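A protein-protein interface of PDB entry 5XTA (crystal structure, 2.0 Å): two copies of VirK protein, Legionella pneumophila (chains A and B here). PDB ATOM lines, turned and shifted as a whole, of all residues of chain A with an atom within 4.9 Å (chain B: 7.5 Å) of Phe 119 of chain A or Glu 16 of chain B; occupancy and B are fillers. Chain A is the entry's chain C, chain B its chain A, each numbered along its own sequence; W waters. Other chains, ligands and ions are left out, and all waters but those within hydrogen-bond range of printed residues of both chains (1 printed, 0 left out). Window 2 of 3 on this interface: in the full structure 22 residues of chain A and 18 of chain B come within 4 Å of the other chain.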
ATOM      1  N   VAL A   2     -24.722   3.069  -4.198  1.00  0.00           N
ATOM      2  CA  VAL A   2     -23.770   4.130  -3.856  1.00  0.00           C
ATOM      3  C   VAL A   2     -22.967   4.483  -5.082  1.00  0.00           C
ATOM      4  O   VAL A   2     -23.020   3.780  -6.076  1.00  0.00           O
ATOM      5  CB  VAL A   2     -22.811   3.703  -2.722  1.00  0.00           C
ATOM      6  CG1 VAL A   2     -23.617   3.330  -1.488  1.00  0.00           C
ATOM      7  CG2 VAL A   2     -21.925   2.531  -3.144  1.00  0.00           C
ATOM      8  N   GLU A   3     -22.195   5.554  -4.989  1.00  0.00           N
ATOM      9  CA  GLU A   3     -21.264   5.911  -6.055  1.00  0.00           C
ATOM     10  C   GLU A   3     -20.176   4.834  -6.215  1.00  0.00           C
ATOM     11  O   GLU A   3     -19.657   4.322  -5.221  1.00  0.00           O
ATOM     12  CB  GLU A   3     -20.643   7.280  -5.801  1.00  0.00           C
ATOM     13  CG  GLU A   3     -19.747   7.712  -6.947  1.00  0.00           C
ATOM     14  CD  GLU A   3     -19.477   9.205  -7.044  1.00  0.00           C
ATOM     15  OE1 GLU A   3     -19.826   9.961  -6.114  1.00  0.00           O
ATOM     16  OE2 GLU A   3     -18.880   9.610  -8.076  1.00  0.00           O
ATOM     17  N   LEU A   4     -19.873   4.469  -7.458  1.00  0.00           N
ATOM     18  CA  LEU A   4     -18.887   3.445  -7.758  1.00  0.00           C
ATOM     19  C   LEU A   4     -17.692   4.226  -8.240  1.00  0.00           C
ATOM     20  O   LEU A   4     -17.636   4.683  -9.393  1.00  0.00           O
ATOM     21  CB  LEU A   4     -19.389   2.421  -8.790  1.00  0.00           C
ATOM     22  CG  LEU A   4     -20.676   1.685  -8.335  1.00  0.00           C
ATOM     23  CD1 LEU A   4     -21.327   0.881  -9.451  1.00  0.00           C
ATOM     24  CD2 LEU A   4     -20.457   0.796  -7.102  1.00  0.00           C
ATOM     25  N   ARG A  19     -27.867  -3.139 -10.848  1.00  0.00           N
ATOM     26  CA  ARG A  19     -28.282  -2.302 -11.960  1.00  0.00           C
ATOM     27  C   ARG A  19     -27.500  -0.984 -11.857  1.00  0.00           C
ATOM     28  O   ARG A  19     -27.429  -0.356 -10.793  1.00  0.00           O
ATOM     29  CB  ARG A  19     -29.816  -2.091 -11.989  1.00  0.00           C
ATOM     30  CG  ARG A  19     -30.219  -1.334 -13.243  1.00  0.00           C
ATOM     31  CD  ARG A  19     -31.611  -1.645 -13.742  1.00  0.00           C
ATOM     32  NE  ARG A  19     -32.010  -0.687 -14.783  1.00  0.00           N
ATOM     33  CZ  ARG A  19     -33.199  -0.638 -15.377  1.00  0.00           C
ATOM     34  NH1 ARG A  19     -34.148  -1.466 -15.006  1.00  0.00           N
ATOM     35  NH2 ARG A  19     -33.444   0.281 -16.304  1.00  0.00           N
ATOM     36  N   ILE A  20     -26.881  -0.594 -12.963  1.00  0.00           N
ATOM     37  CA  ILE A  20     -26.018   0.598 -13.032  1.00  0.00           C
ATOM     38  C   ILE A  20     -26.732   1.902 -13.487  1.00  0.00           C
ATOM     39  O   ILE A  20     -27.526   1.892 -14.441  1.00  0.00           O
ATOM     40  CB  ILE A  20     -24.823   0.280 -13.980  1.00  0.00           C
ATOM     41  CG1 ILE A  20     -23.980  -0.896 -13.441  1.00  0.00           C
ATOM     42  CG2 ILE A  20     -23.930   1.476 -14.192  1.00  0.00           C
ATOM     43  CD1 ILE A  20     -23.714  -0.876 -11.950  1.00  0.00           C
ATOM     44  N   THR A  21     -26.402   3.034 -12.853  1.00  0.00           N
ATOM     45  CA  THR A  21     -26.889   4.328 -13.285  1.00  0.00           C
ATOM     46  C   THR A  21     -25.707   5.243 -13.637  1.00  0.00           C
ATOM     47  O   THR A  21     -24.717   5.340 -12.878  1.00  0.00           O
ATOM     48  CB  THR A  21     -27.837   4.945 -12.237  1.00  0.00           C
ATOM     49  OG1 THR A  21     -28.933   4.033 -12.029  1.00  0.00           O
ATOM     50  CG2 THR A  21     -28.385   6.280 -12.694  1.00  0.00           C
ATOM     51  N   VAL A  23     -24.576   9.125 -14.469  1.00  0.00           N
ATOM     52  CA  VAL A  23     -24.935  10.517 -14.234  1.00  0.00           C
ATOM     53  C   VAL A  23     -23.855  11.389 -14.870  1.00  0.00           C
ATOM     54  O   VAL A  23     -22.677  11.303 -14.502  1.00  0.00           O
ATOM     55  CB  VAL A  23     -25.148  10.851 -12.744  1.00  0.00           C
ATOM     56  CG1 VAL A  23     -25.550  12.315 -12.592  1.00  0.00           C
ATOM     57  CG2 VAL A  23     -26.231   9.953 -12.124  1.00  0.00           C
ATOM     58  N   LYS A 117     -20.233  10.059 -13.750  1.00  0.00           N
ATOM     59  CA  LYS A 117     -20.344   9.346 -12.490  1.00  0.00           C
ATOM     60  C   LYS A 117     -21.236   8.140 -12.641  1.00  0.00           C
ATOM     61  O   LYS A 117     -22.157   8.125 -13.477  1.00  0.00           O
ATOM     62  CB  LYS A 117     -20.886  10.267 -11.416  1.00  0.00           C
ATOM     63  CG  LYS A 117     -19.883  11.363 -11.006  1.00  0.00           C
ATOM     64  CD  LYS A 117     -20.383  12.065  -9.755  1.00  0.00           C
ATOM     65  CE  LYS A 117     -19.573  13.297  -9.411  1.00  0.00           C
ATOM     66  NZ  LYS A 117     -20.230  13.969  -8.253  1.00  0.00           N
ATOM     67  N   VAL A 118     -20.945   7.130 -11.839  1.00  0.00           N
ATOM     68  CA  VAL A 118     -21.587   5.828 -11.975  1.00  0.00           C
ATOM     69  C   VAL A 118     -22.019   5.375 -10.579  1.00  0.00           C
ATOM     70  O   VAL A 118     -21.215   5.407  -9.639  1.00  0.00           O
ATOM     71  CB  VAL A 118     -20.662   4.778 -12.632  1.00  0.00           C
ATOM     72  CG1 VAL A 118     -21.436   3.517 -12.926  1.00  0.00           C
ATOM     73  CG2 VAL A 118     -20.002   5.266 -13.911  1.00  0.00           C
ATOM     74  N   PHE A 119     -23.283   4.953 -10.480  1.00  0.00           N
ATOM     75  CA  PHE A 119     -23.922   4.482  -9.246  1.00  0.00           C
ATOM     76  C   PHE A 119     -24.504   3.069  -9.402  1.00  0.00           C
ATOM     77  O   PHE A 119     -24.969   2.663 -10.489  1.00  0.00           O
ATOM     78  CB  PHE A 119     -25.007   5.446  -8.777  1.00  0.00           C
ATOM     79  CG  PHE A 119     -24.523   6.844  -8.578  1.00  0.00           C
ATOM     80  CD1 PHE A 119     -24.254   7.320  -7.302  1.00  0.00           C
ATOM     81  CD2 PHE A 119     -24.289   7.662  -9.666  1.00  0.00           C
ATOM     82  CE1 PHE A 119     -23.776   8.602  -7.121  1.00  0.00           C
ATOM     83  CE2 PHE A 119     -23.817   8.946  -9.496  1.00  0.00           C
ATOM     84  CZ  PHE A 119     -23.559   9.416  -8.222  1.00  0.00           C
ATOM     85  N   GLY A 120     -24.421   2.299  -8.322  1.00  0.00           N
ATOM     86  CA  GLY A 120     -24.901   0.908  -8.316  1.00  0.00           C
ATOM     87  C   GLY A 120     -24.960   0.298  -6.911  1.00  0.00           C
ATOM     88  O   GLY A 120     -24.186   0.657  -6.010  1.00  0.00           O
ATOM     89  OXT GLY A 120     -25.814  -0.563  -6.632  1.00  0.00           O
ATOM     90  N   GLN B   8     -34.788  21.302  -4.788  1.00  0.00           N
ATOM     91  CA  GLN B   8     -33.411  20.941  -4.472  1.00  0.00           C
ATOM     92  C   GLN B   8     -33.253  19.471  -4.059  1.00  0.00           C
ATOM     93  O   GLN B   8     -32.240  18.853  -4.377  1.00  0.00           O
ATOM     94  CB  GLN B   8     -32.826  21.844  -3.368  1.00  0.00           C
ATOM     95  CG  GLN B   8     -31.308  21.733  -3.219  1.00  0.00           C
ATOM     96  CD  GLN B   8     -30.577  22.147  -4.492  1.00  0.00           C
ATOM     97  OE1 GLN B   8     -30.860  23.193  -5.068  1.00  0.00           O
ATOM     98  NE2 GLN B   8     -29.668  21.309  -4.962  1.00  0.00           N
ATOM     99  N   ASN B   9     -34.218  18.910  -3.331  1.00  0.00           N
ATOM    100  CA  ASN B   9     -34.154  17.503  -2.967  1.00  0.00           C
ATOM    101  C   ASN B   9     -34.127  16.672  -4.236  1.00  0.00           C
ATOM    102  O   ASN B   9     -33.472  15.659  -4.295  1.00  0.00           O
ATOM    103  CB  ASN B   9     -35.356  17.058  -2.125  1.00  0.00           C
ATOM    104  CG  ASN B   9     -35.332  17.591  -0.678  1.00  0.00           C
ATOM    105  OD1 ASN B   9     -34.276  17.891  -0.107  1.00  0.00           O
ATOM    106  ND2 ASN B   9     -36.483  17.645  -0.070  1.00  0.00           N
ATOM    107  N   ILE B  10     -34.897  17.072  -5.231  1.00  0.00           N
ATOM    108  CA  ILE B  10     -35.053  16.265  -6.448  1.00  0.00           C
ATOM    109  C   ILE B  10     -33.772  16.303  -7.272  1.00  0.00           C
ATOM    110  O   ILE B  10     -33.309  15.278  -7.732  1.00  0.00           O
ATOM    111  CB  ILE B  10     -36.244  16.757  -7.301  1.00  0.00           C
ATOM    112  CG1 ILE B  10     -37.562  16.510  -6.554  1.00  0.00           C
ATOM    113  CG2 ILE B  10     -36.258  16.104  -8.696  1.00  0.00           C
ATOM    114  CD1 ILE B  10     -38.755  17.292  -7.098  1.00  0.00           C
ATOM    115  N   VAL B  11     -33.252  17.516  -7.480  1.00  0.00           N
ATOM    116  CA  VAL B  11     -31.974  17.757  -8.142  1.00  0.00           C
ATOM    117  C   VAL B  11     -30.867  16.962  -7.453  1.00  0.00           C
ATOM    118  O   VAL B  11     -30.102  16.279  -8.125  1.00  0.00           O
ATOM    119  CB  VAL B  11     -31.688  19.264  -8.182  1.00  0.00           C
ATOM    120  CG1 VAL B  11     -30.229  19.573  -8.514  1.00  0.00           C
ATOM    121  CG2 VAL B  11     -32.639  19.929  -9.169  1.00  0.00           C
ATOM    122  N   ASP B  12     -30.830  17.004  -6.120  1.00  0.00           N
ATOM    123  CA  ASP B  12     -29.846  16.233  -5.362  1.00  0.00           C
ATOM    124  C   ASP B  12     -29.980  14.715  -5.593  1.00  0.00           C
ATOM    125  O   ASP B  12     -28.964  14.006  -5.701  1.00  0.00           O
ATOM    126  CB  ASP B  12     -29.897  16.559  -3.858  1.00  0.00           C
ATOM    127  CG  ASP B  12     -29.350  17.971  -3.527  1.00  0.00           C
ATOM    128  OD1 ASP B  12     -28.764  18.639  -4.407  1.00  0.00           O
ATOM    129  OD2 ASP B  12     -29.529  18.428  -2.380  1.00  0.00           O
ATOM    130  N   ALA B  13     -31.215  14.220  -5.649  1.00  0.00           N
ATOM    131  CA  ALA B  13     -31.446  12.795  -5.860  1.00  0.00           C
ATOM    132  C   ALA B  13     -30.965  12.354  -7.257  1.00  0.00           C
ATOM    133  O   ALA B  13     -30.384  11.283  -7.424  1.00  0.00           O
ATOM    134  CB  ALA B  13     -32.913  12.457  -5.652  1.00  0.00           C
ATOM    135  N   ILE B  14     -31.187  13.211  -8.242  1.00  0.00           N
ATOM    136  CA  ILE B  14     -30.746  12.919  -9.598  1.00  0.00           C
ATOM    137  C   ILE B  14     -29.208  12.858  -9.647  1.00  0.00           C
ATOM    138  O   ILE B  14     -28.611  11.892 -10.168  1.00  0.00           O
ATOM    139  CB  ILE B  14     -31.317  13.929 -10.599  1.00  0.00           C
ATOM    140  CG1 ILE B  14     -32.829  13.791 -10.658  1.00  0.00           C
ATOM    141  CG2 ILE B  14     -30.699  13.719 -12.000  1.00  0.00           C
ATOM    142  CD1 ILE B  14     -33.520  14.974 -11.274  1.00  0.00           C
ATOM    143  N   ALA B  15     -28.574  13.845  -9.037  1.00  0.00           N
ATOM    144  CA  ALA B  15     -27.131  13.955  -9.043  1.00  0.00           C
ATOM    145  C   ALA B  15     -26.472  12.781  -8.315  1.00  0.00           C
ATOM    146  O   ALA B  15     -25.361  12.406  -8.650  1.00  0.00           O
ATOM    147  CB  ALA B  15     -26.694  15.297  -8.447  1.00  0.00           C
ATOM    148  N   GLU B  16     -27.205  12.178  -7.376  1.00  0.00           N
ATOM    149  CA  GLU B  16     -26.740  11.039  -6.604  1.00  0.00           C
ATOM    150  C   GLU B  16     -27.120   9.711  -7.221  1.00  0.00           C
ATOM    151  O   GLU B  16     -27.013   8.678  -6.561  1.00  0.00           O
ATOM    152  CB  GLU B  16     -27.325  11.079  -5.196  1.00  0.00           C
ATOM    153  CG  GLU B  16     -26.675  12.064  -4.248  1.00  0.00           C
ATOM    154  CD  GLU B  16     -27.590  12.440  -3.076  1.00  0.00           C
ATOM    155  OE1 GLU B  16     -28.466  11.628  -2.682  1.00  0.00           O
ATOM    156  OE2 GLU B  16     -27.452  13.571  -2.559  1.00  0.00           O
ATOM    157  N   GLY B  17     -27.588   9.700  -8.460  1.00  0.00           N
ATOM    158  CA  GLY B  17     -27.867   8.432  -9.097  1.00  0.00           C
ATOM    159  C   GLY B  17     -29.135   7.706  -8.703  1.00  0.00           C
ATOM    160  O   GLY B  17     -29.319   6.595  -9.134  1.00  0.00           O
ATOM    161  N   LYS B  18     -30.067   8.344  -8.016  1.00  0.00           N
ATOM    162  CA  LYS B  18     -31.345   7.702  -7.726  1.00  0.00           C
ATOM    163  C   LYS B  18     -32.324   7.696  -8.933  1.00  0.00           C
ATOM    164  O   LYS B  18     -32.456   8.642  -9.627  1.00  0.00           O
ATOM    165  CB  LYS B  18     -32.005   8.384  -6.569  1.00  0.00           C
ATOM    166  CG  LYS B  18     -31.246   8.158  -5.277  1.00  0.00           C
ATOM    167  CD  LYS B  18     -31.639   9.216  -4.256  1.00  0.00           C
ATOM    168  CE  LYS B  18     -30.915   9.061  -2.910  1.00  0.00           C
ATOM    169  NZ  LYS B  18     -31.518   7.988  -2.085  1.00  0.00           N
ATOM    170  N   ARG B  19     -33.038   6.612  -9.104  1.00  0.00           N
ATOM    171  CA  ARG B  19     -34.087   6.545 -10.106  1.00  0.00           C
ATOM    172  C   ARG B  19     -35.364   7.223  -9.566  1.00  0.00           C
ATOM    173  O   ARG B  19     -35.802   6.946  -8.474  1.00  0.00           O
ATOM    174  CB  ARG B  19     -34.329   5.103 -10.508  1.00  0.00           C
ATOM    175  CG  ARG B  19     -35.360   5.031 -11.631  1.00  0.00           C
ATOM    176  CD  ARG B  19     -35.188   3.837 -12.533  1.00  0.00           C
ATOM    177  NE  ARG B  19     -36.278   3.781 -13.520  1.00  0.00           N
ATOM    178  CZ  ARG B  19     -36.457   2.784 -14.370  1.00  0.00           C
ATOM    179  NH1 ARG B  19     -35.625   1.755 -14.321  1.00  0.00           N
ATOM    180  NH2 ARG B  19     -37.467   2.816 -15.261  1.00  0.00           N
HETATM  181  O   HOH W   1     -23.292  13.054  -6.874  1.00  0.00           O
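NH1 of Arg 19 of chain B lies close to NH2 of Arg 19 of chain A (3.3 Å).
O of Phe 119 of chain A lies within hydrogen-bond range of N of Thr 21 of chain A (2.8 Å).
N of Val 23 of chain A lies within hydrogen-bond range of O of Lys 117 of chain A, at 2.8 Å.
Gly 17 of chain B touches Thr 21 of chain A (O to CG2, 3.7 Å).
O of Ile 14 of chain B touches CG2 of Val 23 of chain A, at 3.6 Å.
Val 23 of chain A touches Ala 15 of chain B (CG1 to O, 3.9 Å).
Val 23 of chain A touches Gly 17 of chain B.
Phe 119 of chain A touches Ala 15 of chain B (CZ to O, 3.5 Å).
Glu 16 of chain B touches Phe 119 of chain A.
Gly 17 of chain B touches Phe 119 of chain A.
Of the printed residues of chain B, Arg 19 of chain A touches Arg 19 (3.3 Å).
Of the printed residues of chain B, Thr 21 of chain A touches Gly 17 (3.7 Å).
Of the printed residues of chain B, Val 23 of chain A touches Ile 14 (3.6 Å), Ala 15 (3.9 Å) and Gly 17 (3.8 Å).
Of chain B, only Ala 15 (3.5 Å), Glu 16 (3.2 Å) and Gly 17 (3.7 Å) come within 4 Å of Phe 119 of chain A.
Of the printed residues of chain A, Ile 14 of chain B touches Val 23 (3.6 Å).
Glu 16 of chain B touches one residue of chain A.
Of the printed residues of chain A, Gly 17 of chain B touches Thr 21 (3.7 Å), Val 23 (3.8 Å) and Phe 119 (3.7 Å).
Lys 18 of chain B touches none of the printed residues of chain A.
The nearest residue of chain B that does not touch Phe 119 of chain A is Ile 14 of chain B (5.7 Å).
The nearest printed residue of chain A that does not touch Glu 16 of chain B is Val 23 of chain A (5.0 Å).
Of the 11 printed residues of chain A, 4 touch a printed residue of chain B.
Printed residues of chain A that touch a printed residue of chain B: Arg 19, Thr 21, Val 23 and Phe 119.
Hydrophobic or aromatic side chains of chain A that line the printed part of chain B: Val 23 and Phe 119.
Of the 12 printed residues of chain B, 5 touch a printed residue of chain A.
Among the printed residues, 8 pairs touch across the chains.
Among the printed residues, no Asp or Glu carboxylate lies within 4 Å of a Lys or Arg side-chain nitrogen of the other chain.
Arg 19 of chain B touches its own counterpart, Arg 19 of chain A.
Position printed for both chains: 19.
Of the 8 pairs that touch across the chains among the printed residues, 1 has its exchanged pair printed and touching as well.
Water W1 bridges the backbone carbonyl oxygen (O) of Ala 15 of chain B and the side-chain amino group (NZ) of Lys 117 of chain A.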
